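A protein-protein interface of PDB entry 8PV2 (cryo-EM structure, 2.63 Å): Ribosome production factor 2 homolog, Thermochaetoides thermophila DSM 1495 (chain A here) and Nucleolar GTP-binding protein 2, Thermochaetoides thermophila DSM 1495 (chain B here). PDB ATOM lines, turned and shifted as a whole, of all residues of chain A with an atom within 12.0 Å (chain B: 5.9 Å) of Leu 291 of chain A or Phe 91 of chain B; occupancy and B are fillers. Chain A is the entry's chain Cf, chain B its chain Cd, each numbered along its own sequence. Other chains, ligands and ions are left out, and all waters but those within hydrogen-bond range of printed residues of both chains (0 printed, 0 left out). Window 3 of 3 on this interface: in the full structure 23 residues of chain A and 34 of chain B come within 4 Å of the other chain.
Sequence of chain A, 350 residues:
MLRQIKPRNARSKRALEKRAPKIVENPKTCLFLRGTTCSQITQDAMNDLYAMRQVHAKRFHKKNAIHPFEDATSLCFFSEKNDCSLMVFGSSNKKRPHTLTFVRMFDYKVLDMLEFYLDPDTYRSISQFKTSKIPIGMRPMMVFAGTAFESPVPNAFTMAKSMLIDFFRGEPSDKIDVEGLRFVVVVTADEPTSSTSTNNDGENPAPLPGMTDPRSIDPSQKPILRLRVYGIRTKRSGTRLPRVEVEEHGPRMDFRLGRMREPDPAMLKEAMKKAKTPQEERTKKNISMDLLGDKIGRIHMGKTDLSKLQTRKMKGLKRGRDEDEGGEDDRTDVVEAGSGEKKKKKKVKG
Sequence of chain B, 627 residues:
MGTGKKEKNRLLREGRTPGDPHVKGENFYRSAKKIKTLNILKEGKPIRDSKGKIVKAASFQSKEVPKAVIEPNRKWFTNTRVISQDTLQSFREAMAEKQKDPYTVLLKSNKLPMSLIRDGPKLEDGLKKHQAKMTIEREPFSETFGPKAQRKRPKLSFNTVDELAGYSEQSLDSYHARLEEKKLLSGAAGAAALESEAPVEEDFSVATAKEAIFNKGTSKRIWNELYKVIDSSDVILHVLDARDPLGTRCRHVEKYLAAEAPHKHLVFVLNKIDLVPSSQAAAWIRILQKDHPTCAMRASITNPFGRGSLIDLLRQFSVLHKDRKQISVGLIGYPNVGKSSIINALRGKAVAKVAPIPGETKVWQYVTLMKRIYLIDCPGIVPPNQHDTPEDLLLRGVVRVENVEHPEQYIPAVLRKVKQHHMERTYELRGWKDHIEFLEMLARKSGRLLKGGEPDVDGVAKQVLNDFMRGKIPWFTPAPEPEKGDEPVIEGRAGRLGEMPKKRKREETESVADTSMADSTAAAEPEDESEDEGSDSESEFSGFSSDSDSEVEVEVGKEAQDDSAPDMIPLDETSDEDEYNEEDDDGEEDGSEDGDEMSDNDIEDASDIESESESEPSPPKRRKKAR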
ATOM      1  N   GLU A 281     -24.580 -19.595   0.509  1.00  0.00           N
ATOM      2  CA  GLU A 281     -23.476 -20.542   0.564  1.00  0.00           C
ATOM      3  C   GLU A 281     -23.931 -21.873   1.145  1.00  0.00           C
ATOM      4  O   GLU A 281     -24.599 -21.916   2.183  1.00  0.00           O
ATOM      5  CB  GLU A 281     -22.332 -19.974   1.398  1.00  0.00           C
ATOM      6  CG  GLU A 281     -21.143 -20.906   1.518  1.00  0.00           C
ATOM      7  CD  GLU A 281     -19.981 -20.279   2.252  1.00  0.00           C
ATOM      8  OE1 GLU A 281     -20.149 -19.167   2.795  1.00  0.00           O
ATOM      9  OE2 GLU A 281     -18.900 -20.900   2.292  1.00  0.00           O
ATOM     10  N   ILE A 287     -15.787 -25.691   8.031  1.00  0.00           N
ATOM     11  CA  ILE A 287     -15.292 -24.620   7.176  1.00  0.00           C
ATOM     12  C   ILE A 287     -16.143 -23.393   7.443  1.00  0.00           C
ATOM     13  O   ILE A 287     -17.376 -23.476   7.437  1.00  0.00           O
ATOM     14  CB  ILE A 287     -15.352 -24.995   5.685  1.00  0.00           C
ATOM     15  CG1 ILE A 287     -14.668 -26.334   5.428  1.00  0.00           C
ATOM     16  CG2 ILE A 287     -14.707 -23.910   4.841  1.00  0.00           C
ATOM     17  CD1 ILE A 287     -13.202 -26.304   5.666  1.00  0.00           C
ATOM     18  N   SER A 288     -15.494 -22.259   7.675  1.00  0.00           N
ATOM     19  CA  SER A 288     -16.230 -21.028   7.901  1.00  0.00           C
ATOM     20  C   SER A 288     -15.485 -19.877   7.247  1.00  0.00           C
ATOM     21  O   SER A 288     -14.380 -20.036   6.730  1.00  0.00           O
ATOM     22  CB  SER A 288     -16.440 -20.770   9.395  1.00  0.00           C
ATOM     23  OG  SER A 288     -15.212 -20.483  10.039  1.00  0.00           O
ATOM     24  N   MET A 289     -16.120 -18.715   7.257  1.00  0.00           N
ATOM     25  CA  MET A 289     -15.507 -17.466   6.838  1.00  0.00           C
ATOM     26  C   MET A 289     -15.515 -16.526   8.032  1.00  0.00           C
ATOM     27  O   MET A 289     -16.562 -16.326   8.652  1.00  0.00           O
ATOM     28  CB  MET A 289     -16.270 -16.855   5.663  1.00  0.00           C
ATOM     29  CG  MET A 289     -15.683 -15.578   5.120  1.00  0.00           C
ATOM     30  SD  MET A 289     -16.629 -14.946   3.725  1.00  0.00           S
ATOM     31  CE  MET A 289     -18.109 -14.366   4.542  1.00  0.00           C
ATOM     32  N   ASP A 290     -14.359 -15.961   8.367  1.00  0.00           N
ATOM     33  CA  ASP A 290     -14.357 -15.101   9.543  1.00  0.00           C
ATOM     34  C   ASP A 290     -14.813 -13.698   9.149  1.00  0.00           C
ATOM     35  O   ASP A 290     -15.334 -13.466   8.056  1.00  0.00           O
ATOM     36  CB  ASP A 290     -12.986 -15.067  10.212  1.00  0.00           C
ATOM     37  CG  ASP A 290     -11.911 -14.574   9.300  1.00  0.00           C
ATOM     38  OD1 ASP A 290     -10.944 -13.956   9.788  1.00  0.00           O
ATOM     39  OD2 ASP A 290     -12.070 -14.732   8.084  1.00  0.00           O
ATOM     40  N   LEU A 291     -14.619 -12.739  10.054  1.00  0.00           N
ATOM     41  CA  LEU A 291     -15.078 -11.385   9.780  1.00  0.00           C
ATOM     42  C   LEU A 291     -14.187 -10.655   8.786  1.00  0.00           C
ATOM     43  O   LEU A 291     -14.625  -9.663   8.197  1.00  0.00           O
ATOM     44  CB  LEU A 291     -15.179 -10.592  11.080  1.00  0.00           C
ATOM     45  CG  LEU A 291     -16.365 -10.950  11.974  1.00  0.00           C
ATOM     46  CD1 LEU A 291     -16.405 -10.057  13.198  1.00  0.00           C
ATOM     47  CD2 LEU A 291     -17.664 -10.852  11.195  1.00  0.00           C
ATOM     48  N   LEU A 292     -12.959 -11.122   8.578  1.00  0.00           N
ATOM     49  CA  LEU A 292     -12.052 -10.528   7.609  1.00  0.00           C
ATOM     50  C   LEU A 292     -12.102 -11.222   6.257  1.00  0.00           C
ATOM     51  O   LEU A 292     -11.348 -10.853   5.354  1.00  0.00           O
ATOM     52  CB  LEU A 292     -10.622 -10.540   8.145  1.00  0.00           C
ATOM     53  CG  LEU A 292     -10.296  -9.479   9.192  1.00  0.00           C
ATOM     54  CD1 LEU A 292      -8.959  -9.770   9.829  1.00  0.00           C
ATOM     55  CD2 LEU A 292     -10.291  -8.104   8.565  1.00  0.00           C
ATOM     56  N   GLY A 293     -12.973 -12.211   6.093  1.00  0.00           N
ATOM     57  CA  GLY A 293     -13.138 -12.877   4.824  1.00  0.00           C
ATOM     58  C   GLY A 293     -12.250 -14.075   4.591  1.00  0.00           C
ATOM     59  O   GLY A 293     -12.329 -14.680   3.516  1.00  0.00           O
ATOM     60  N   ASP A 294     -11.411 -14.438   5.552  1.00  0.00           N
ATOM     61  CA  ASP A 294     -10.566 -15.612   5.409  1.00  0.00           C
ATOM     62  C   ASP A 294     -11.380 -16.882   5.602  1.00  0.00           C
ATOM     63  O   ASP A 294     -12.332 -16.929   6.391  1.00  0.00           O
ATOM     64  CB  ASP A 294      -9.424 -15.584   6.422  1.00  0.00           C
ATOM     65  CG  ASP A 294      -8.536 -14.370   6.272  1.00  0.00           C
ATOM     66  OD1 ASP A 294      -8.550 -13.745   5.195  1.00  0.00           O
ATOM     67  OD2 ASP A 294      -7.817 -14.040   7.237  1.00  0.00           O
ATOM     68  N   LYS A 295     -11.000 -17.917   4.860  1.00  0.00           N
ATOM     69  CA  LYS A 295     -11.560 -19.244   5.057  1.00  0.00           C
ATOM     70  C   LYS A 295     -10.824 -19.933   6.197  1.00  0.00           C
ATOM     71  O   LYS A 295      -9.593 -20.020   6.193  1.00  0.00           O
ATOM     72  CB  LYS A 295     -11.458 -20.064   3.772  1.00  0.00           C
ATOM     73  CG  LYS A 295     -12.096 -21.429   3.871  1.00  0.00           C
ATOM     74  CD  LYS A 295     -11.977 -22.194   2.570  1.00  0.00           C
ATOM     75  CE  LYS A 295     -12.754 -21.513   1.470  1.00  0.00           C
ATOM     76  NZ  LYS A 295     -12.639 -22.234   0.177  1.00  0.00           N
ATOM     77  N   ILE A 296     -11.583 -20.420   7.172  1.00  0.00           N
ATOM     78  CA  ILE A 296     -11.057 -20.932   8.428  1.00  0.00           C
ATOM     79  C   ILE A 296     -11.503 -22.375   8.595  1.00  0.00           C
ATOM     80  O   ILE A 296     -12.677 -22.700   8.380  1.00  0.00           O
ATOM     81  CB  ILE A 296     -11.530 -20.074   9.621  1.00  0.00           C
ATOM     82  CG1 ILE A 296     -11.176 -18.606   9.401  1.00  0.00           C
ATOM     83  CG2 ILE A 296     -10.923 -20.561  10.910  1.00  0.00           C
ATOM     84  CD1 ILE A 296      -9.701 -18.358   9.258  1.00  0.00           C
ATOM     85  N   GLY A 297     -10.567 -23.239   8.974  1.00  0.00           N
ATOM     86  CA  GLY A 297     -10.853 -24.632   9.256  1.00  0.00           C
ATOM     87  C   GLY A 297     -10.767 -24.924  10.741  1.00  0.00           C
ATOM     88  O   GLY A 297      -9.908 -24.391  11.443  1.00  0.00           O
ATOM     89  N   ILE B  83     -12.674  -0.602  -3.276  1.00  0.00           N
ATOM     90  CA  ILE B  83     -13.277  -0.870  -1.978  1.00  0.00           C
ATOM     91  C   ILE B  83     -13.891   0.424  -1.463  1.00  0.00           C
ATOM     92  O   ILE B  83     -13.395   1.518  -1.750  1.00  0.00           O
ATOM     93  CB  ILE B  83     -12.244  -1.473  -0.994  1.00  0.00           C
ATOM     94  CG1 ILE B  83     -12.924  -2.025   0.260  1.00  0.00           C
ATOM     95  CG2 ILE B  83     -11.146  -0.477  -0.645  1.00  0.00           C
ATOM     96  CD1 ILE B  83     -12.048  -2.937   1.068  1.00  0.00           C
ATOM     97  N   ASP B  86     -17.276   2.246   3.830  1.00  0.00           N
ATOM     98  CA  ASP B  86     -18.025   1.424   4.776  1.00  0.00           C
ATOM     99  C   ASP B  86     -17.394   0.046   4.930  1.00  0.00           C
ATOM    100  O   ASP B  86     -17.268  -0.469   6.049  1.00  0.00           O
ATOM    101  CB  ASP B  86     -19.473   1.294   4.318  1.00  0.00           C
ATOM    102  CG  ASP B  86     -20.235   2.598   4.418  1.00  0.00           C
ATOM    103  OD1 ASP B  86     -19.900   3.421   5.294  1.00  0.00           O
ATOM    104  OD2 ASP B  86     -21.170   2.801   3.618  1.00  0.00           O
ATOM    105  N   THR B  87     -16.988  -0.556   3.811  1.00  0.00           N
ATOM    106  CA  THR B  87     -16.333  -1.857   3.850  1.00  0.00           C
ATOM    107  C   THR B  87     -14.994  -1.774   4.571  1.00  0.00           C
ATOM    108  O   THR B  87     -14.656  -2.657   5.371  1.00  0.00           O
ATOM    109  CB  THR B  87     -16.155  -2.379   2.428  1.00  0.00           C
ATOM    110  OG1 THR B  87     -17.419  -2.355   1.757  1.00  0.00           O
ATOM    111  CG2 THR B  87     -15.652  -3.797   2.443  1.00  0.00           C
ATOM    112  N   LEU B  88     -14.235  -0.700   4.324  1.00  0.00           N
ATOM    113  CA  LEU B  88     -12.980  -0.496   5.040  1.00  0.00           C
ATOM    114  C   LEU B  88     -13.203  -0.345   6.536  1.00  0.00           C
ATOM    115  O   LEU B  88     -12.447  -0.899   7.337  1.00  0.00           O
ATOM    116  CB  LEU B  88     -12.247   0.725   4.496  1.00  0.00           C
ATOM    117  CG  LEU B  88     -11.369   0.491   3.273  1.00  0.00           C
ATOM    118  CD1 LEU B  88     -10.902   1.812   2.704  1.00  0.00           C
ATOM    119  CD2 LEU B  88     -10.189  -0.382   3.642  1.00  0.00           C
ATOM    120  N   GLN B  89     -14.240   0.396   6.937  1.00  0.00           N
ATOM    121  CA  GLN B  89     -14.486   0.605   8.360  1.00  0.00           C
ATOM    122  C   GLN B  89     -14.927  -0.687   9.043  1.00  0.00           C
ATOM    123  O   GLN B  89     -14.528  -0.964  10.183  1.00  0.00           O
ATOM    124  CB  GLN B  89     -15.523   1.711   8.551  1.00  0.00           C
ATOM    125  CG  GLN B  89     -15.825   2.035  10.003  1.00  0.00           C
ATOM    126  CD  GLN B  89     -14.606   2.529  10.763  1.00  0.00           C
ATOM    127  OE1 GLN B  89     -13.737   3.198  10.206  1.00  0.00           O
ATOM    128  NE2 GLN B  89     -14.533   2.188  12.044  1.00  0.00           N
ATOM    129  N   SER B  90     -15.736  -1.497   8.354  1.00  0.00           N
ATOM    130  CA  SER B  90     -16.114  -2.803   8.888  1.00  0.00           C
ATOM    131  C   SER B  90     -14.895  -3.704   9.048  1.00  0.00           C
ATOM    132  O   SER B  90     -14.763  -4.422  10.048  1.00  0.00           O
ATOM    133  CB  SER B  90     -17.151  -3.460   7.982  1.00  0.00           C
ATOM    134  OG  SER B  90     -18.311  -2.657   7.870  1.00  0.00           O
ATOM    135  N   PHE B  91     -13.983  -3.667   8.074  1.00  0.00           N
ATOM    136  CA  PHE B  91     -12.765  -4.461   8.181  1.00  0.00           C
ATOM    137  C   PHE B  91     -11.868  -3.966   9.308  1.00  0.00           C
ATOM    138  O   PHE B  91     -11.196  -4.764   9.966  1.00  0.00           O
ATOM    139  CB  PHE B  91     -12.017  -4.447   6.852  1.00  0.00           C
ATOM    140  CG  PHE B  91     -12.555  -5.419   5.852  1.00  0.00           C
ATOM    141  CD1 PHE B  91     -13.010  -6.661   6.255  1.00  0.00           C
ATOM    142  CD2 PHE B  91     -12.611  -5.092   4.513  1.00  0.00           C
ATOM    143  CE1 PHE B  91     -13.511  -7.557   5.338  1.00  0.00           C
ATOM    144  CE2 PHE B  91     -13.109  -5.988   3.594  1.00  0.00           C
ATOM    145  CZ  PHE B  91     -13.560  -7.220   4.007  1.00  0.00           C
ATOM    146  N   ARG B  92     -11.838  -2.652   9.543  1.00  0.00           N
ATOM    147  CA  ARG B  92     -11.050  -2.115  10.651  1.00  0.00           C
ATOM    148  C   ARG B  92     -11.617  -2.551  11.994  1.00  0.00           C
ATOM    149  O   ARG B  92     -10.864  -2.874  12.923  1.00  0.00           O
ATOM    150  CB  ARG B  92     -10.989  -0.593  10.574  1.00  0.00           C
ATOM    151  CG  ARG B  92     -10.195  -0.061   9.408  1.00  0.00           C
ATOM    152  CD  ARG B  92      -9.905   1.410   9.563  1.00  0.00           C
ATOM    153  NE  ARG B  92      -9.429   1.994   8.317  1.00  0.00           N
ATOM    154  CZ  ARG B  92     -10.145   2.800   7.548  1.00  0.00           C
ATOM    155  NH1 ARG B  92     -11.359   3.187   7.895  1.00  0.00           N
ATOM    156  NH2 ARG B  92      -9.624   3.238   6.407  1.00  0.00           N
ATOM    157  N   GLU B  93     -12.947  -2.561  12.117  1.00  0.00           N
ATOM    158  CA  GLU B  93     -13.571  -3.051  13.343  1.00  0.00           C
ATOM    159  C   GLU B  93     -13.290  -4.533  13.557  1.00  0.00           C
ATOM    160  O   GLU B  93     -13.025  -4.965  14.686  1.00  0.00           O
ATOM    161  CB  GLU B  93     -15.072  -2.788  13.307  1.00  0.00           C
ATOM    162  CG  GLU B  93     -15.429  -1.320  13.348  1.00  0.00           C
ATOM    163  CD  GLU B  93     -16.919  -1.088  13.308  1.00  0.00           C
ATOM    164  OE1 GLU B  93     -17.669  -2.076  13.164  1.00  0.00           O
ATOM    165  OE2 GLU B  93     -17.343   0.081  13.420  1.00  0.00           O
ATOM    166  N   ALA B  94     -13.330  -5.324  12.481  1.00  0.00           N
ATOM    167  CA  ALA B  94     -12.974  -6.737  12.588  1.00  0.00           C
ATOM    168  C   ALA B  94     -11.511  -6.919  12.982  1.00  0.00           C
ATOM    169  O   ALA B  94     -11.175  -7.827  13.753  1.00  0.00           O
ATOM    170  CB  ALA B  94     -13.267  -7.446  11.270  1.00  0.00           C
ATOM    171  N   MET B  95     -10.627  -6.070  12.454  1.00  0.00           N
ATOM    172  CA  MET B  95      -9.209  -6.118  12.798  1.00  0.00           C
ATOM    173  C   MET B  95      -8.990  -5.816  14.274  1.00  0.00           C
ATOM    174  O   MET B  95      -8.147  -6.438  14.931  1.00  0.00           O
ATOM    175  CB  MET B  95      -8.443  -5.121  11.930  1.00  0.00           C
ATOM    176  CG  MET B  95      -6.954  -5.365  11.781  1.00  0.00           C
ATOM    177  SD  MET B  95      -6.514  -6.901  10.962  1.00  0.00           S
ATOM    178  CE  MET B  95      -5.268  -7.506  12.088  1.00  0.00           C
ATOM    179  N   ALA B  96      -9.731  -4.845  14.808  1.00  0.00           N
ATOM    180  CA  ALA B  96      -9.618  -4.542  16.230  1.00  0.00           C
ATOM    181  C   ALA B  96     -10.197  -5.663  17.086  1.00  0.00           C
ATOM    182  O   ALA B  96      -9.683  -5.954  18.172  1.00  0.00           O
ATOM    183  CB  ALA B  96     -10.310  -3.215  16.540  1.00  0.00           C
ATOM    184  N   GLU B  97     -11.266  -6.304  16.613  1.00  0.00           N
ATOM    185  CA  GLU B  97     -11.978  -7.303  17.401  1.00  0.00           C
ATOM    186  C   GLU B  97     -11.339  -8.689  17.341  1.00  0.00           C
ATOM    187  O   GLU B  97     -11.612  -9.512  18.222  1.00  0.00           O
ATOM    188  CB  GLU B  97     -13.442  -7.327  16.921  1.00  0.00           C
ATOM    189  CG  GLU B  97     -14.468  -8.123  17.734  1.00  0.00           C
ATOM    190  CD  GLU B  97     -14.493  -9.596  17.383  1.00  0.00           C
ATOM    191  OE1 GLU B  97     -14.171  -9.931  16.224  1.00  0.00           O
ATOM    192  OE2 GLU B  97     -14.834 -10.417  18.262  1.00  0.00           O
ATOM    193  N   ASN B 110      -7.850 -13.814   2.520  1.00  0.00           N
ATOM    194  CA  ASN B 110      -8.636 -12.890   1.715  1.00  0.00           C
ATOM    195  C   ASN B 110      -7.720 -11.787   1.206  1.00  0.00           C
ATOM    196  O   ASN B 110      -6.989 -11.173   1.989  1.00  0.00           O
ATOM    197  CB  ASN B 110      -9.787 -12.306   2.530  1.00  0.00           C
ATOM    198  CG  ASN B 110     -10.789 -11.570   1.677  1.00  0.00           C
ATOM    199  OD1 ASN B 110     -10.760 -11.658   0.454  1.00  0.00           O
ATOM    200  ND2 ASN B 110     -11.692 -10.851   2.320  1.00  0.00           N
ATOM    201  N   LEU B 112      -6.907  -8.423   0.574  1.00  0.00           N
ATOM    202  CA  LEU B 112      -7.429  -7.183   1.119  1.00  0.00           C
ATOM    203  C   LEU B 112      -6.321  -6.146   1.155  1.00  0.00           C
ATOM    204  O   LEU B 112      -5.140  -6.497   1.238  1.00  0.00           O
ATOM    205  CB  LEU B 112      -7.989  -7.399   2.530  1.00  0.00           C
ATOM    206  CG  LEU B 112      -9.324  -8.122   2.618  1.00  0.00           C
ATOM    207  CD1 LEU B 112      -9.757  -8.220   4.064  1.00  0.00           C
ATOM    208  CD2 LEU B 112     -10.359  -7.399   1.784  1.00  0.00           C
ATOM    209  N   ILE B 117      -6.180  -1.144   6.575  1.00  0.00           N
ATOM    210  CA  ILE B 117      -7.030  -1.849   7.522  1.00  0.00           C
ATOM    211  C   ILE B 117      -6.340  -2.061   8.861  1.00  0.00           C
ATOM    212  O   ILE B 117      -6.959  -1.880   9.916  1.00  0.00           O
ATOM    213  CB  ILE B 117      -7.510  -3.194   6.934  1.00  0.00           C
ATOM    214  CG1 ILE B 117      -8.245  -2.951   5.618  1.00  0.00           C
ATOM    215  CG2 ILE B 117      -8.435  -3.906   7.893  1.00  0.00           C
ATOM    216  CD1 ILE B 117      -8.578  -4.204   4.863  1.00  0.00           C
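The backbone carbonyl oxygen of Leu 292 of chain A is in hydrogen-bond range of the side-chain amide nitrogen of Asn 110 of chain B, at 3.1 Å.
The backbone NH (N) of Asn 110 of chain B lies within hydrogen-bond range of the side-chain carboxylate (OD1) of Asp 294 of chain A (2.8 Å).
The side-chain carboxylate of Asp 290 of chain A is in hydrogen-bond range of the backbone NH of Gly 293 of chain A, at 3.3 Å.
OD2 of Asp 290 of chain A sits at hydrogen-bond distance from N of Asp 294 of chain A (2.6 Å).
Phe 91 of chain B touches Leu 291 of chain A.
Leu 291 of chain A touches Ala 94 of chain B (CB to CB, 3.7 Å).
Leu 291 of chain A touches Glu 97 of chain B.
Phe 91 of chain B touches Leu 292 of chain A (O to CD2, 3.7 Å).
SD of Met 95 of chain B touches CD1 of Leu 292 of chain A, 3.9 Å away.
CD1 of Leu 112 of chain B touches O of Leu 292 of chain A, at 3.3 Å.
ND2 of Asn 110 of chain B touches CA of Gly 293 of chain A, at 3.5 Å.
Printed residues of chain B within 4 Å of Leu 291 of chain A: Phe 91, Ala 94 and Glu 97.
Of the printed residues of chain B, Leu 292 of chain A touches Phe 91, Met 95, Asn 110 and Leu 112.
Of the printed residues of chain B, Gly 293 of chain A touches Asn 110.
Printed residues of chain B within 4 Å of Asp 294 of chain A: Asn 110 (2.8 Å).
Gly 297 of chain A touches none of the printed residues of chain B.
No residue of chain A comes within 4 Å of Thr 87 of chain B.
No residue of chain A comes within 4 Å of Leu 88 of chain B.
Phe 91 of chain B touches just these residues of chain A: Leu 291 and Leu 292.
Of the printed residues of chain A, Met 95 of chain B touches Leu 292.
Printed residues of chain A within 4 Å of Asn 110 of chain B: Leu 292 (3.1 Å), Gly 293 (3.5 Å) and Asp 294 (2.8 Å).
Of the printed residues of chain A, Leu 112 of chain B touches Leu 292.
The nearest residue of chain A that does not touch Phe 91 of chain B is Gly 293 of chain A (4.7 Å).
Hydrophobic or aromatic side chains of chain A within 4 Å of the printed part of chain B: Leu 291 and Leu 292.
Printed residues of chain B that touch a printed residue of chain A: Phe 91, Ala 94, Met 95, Glu 97, Asn 110 and Leu 112.
Among the printed residues, 9 pairs touch across the chains.
Among the printed residues, no Asp or Glu carboxylate lies within 4 Å of a Lys or Arg side-chain nitrogen of the other chain.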
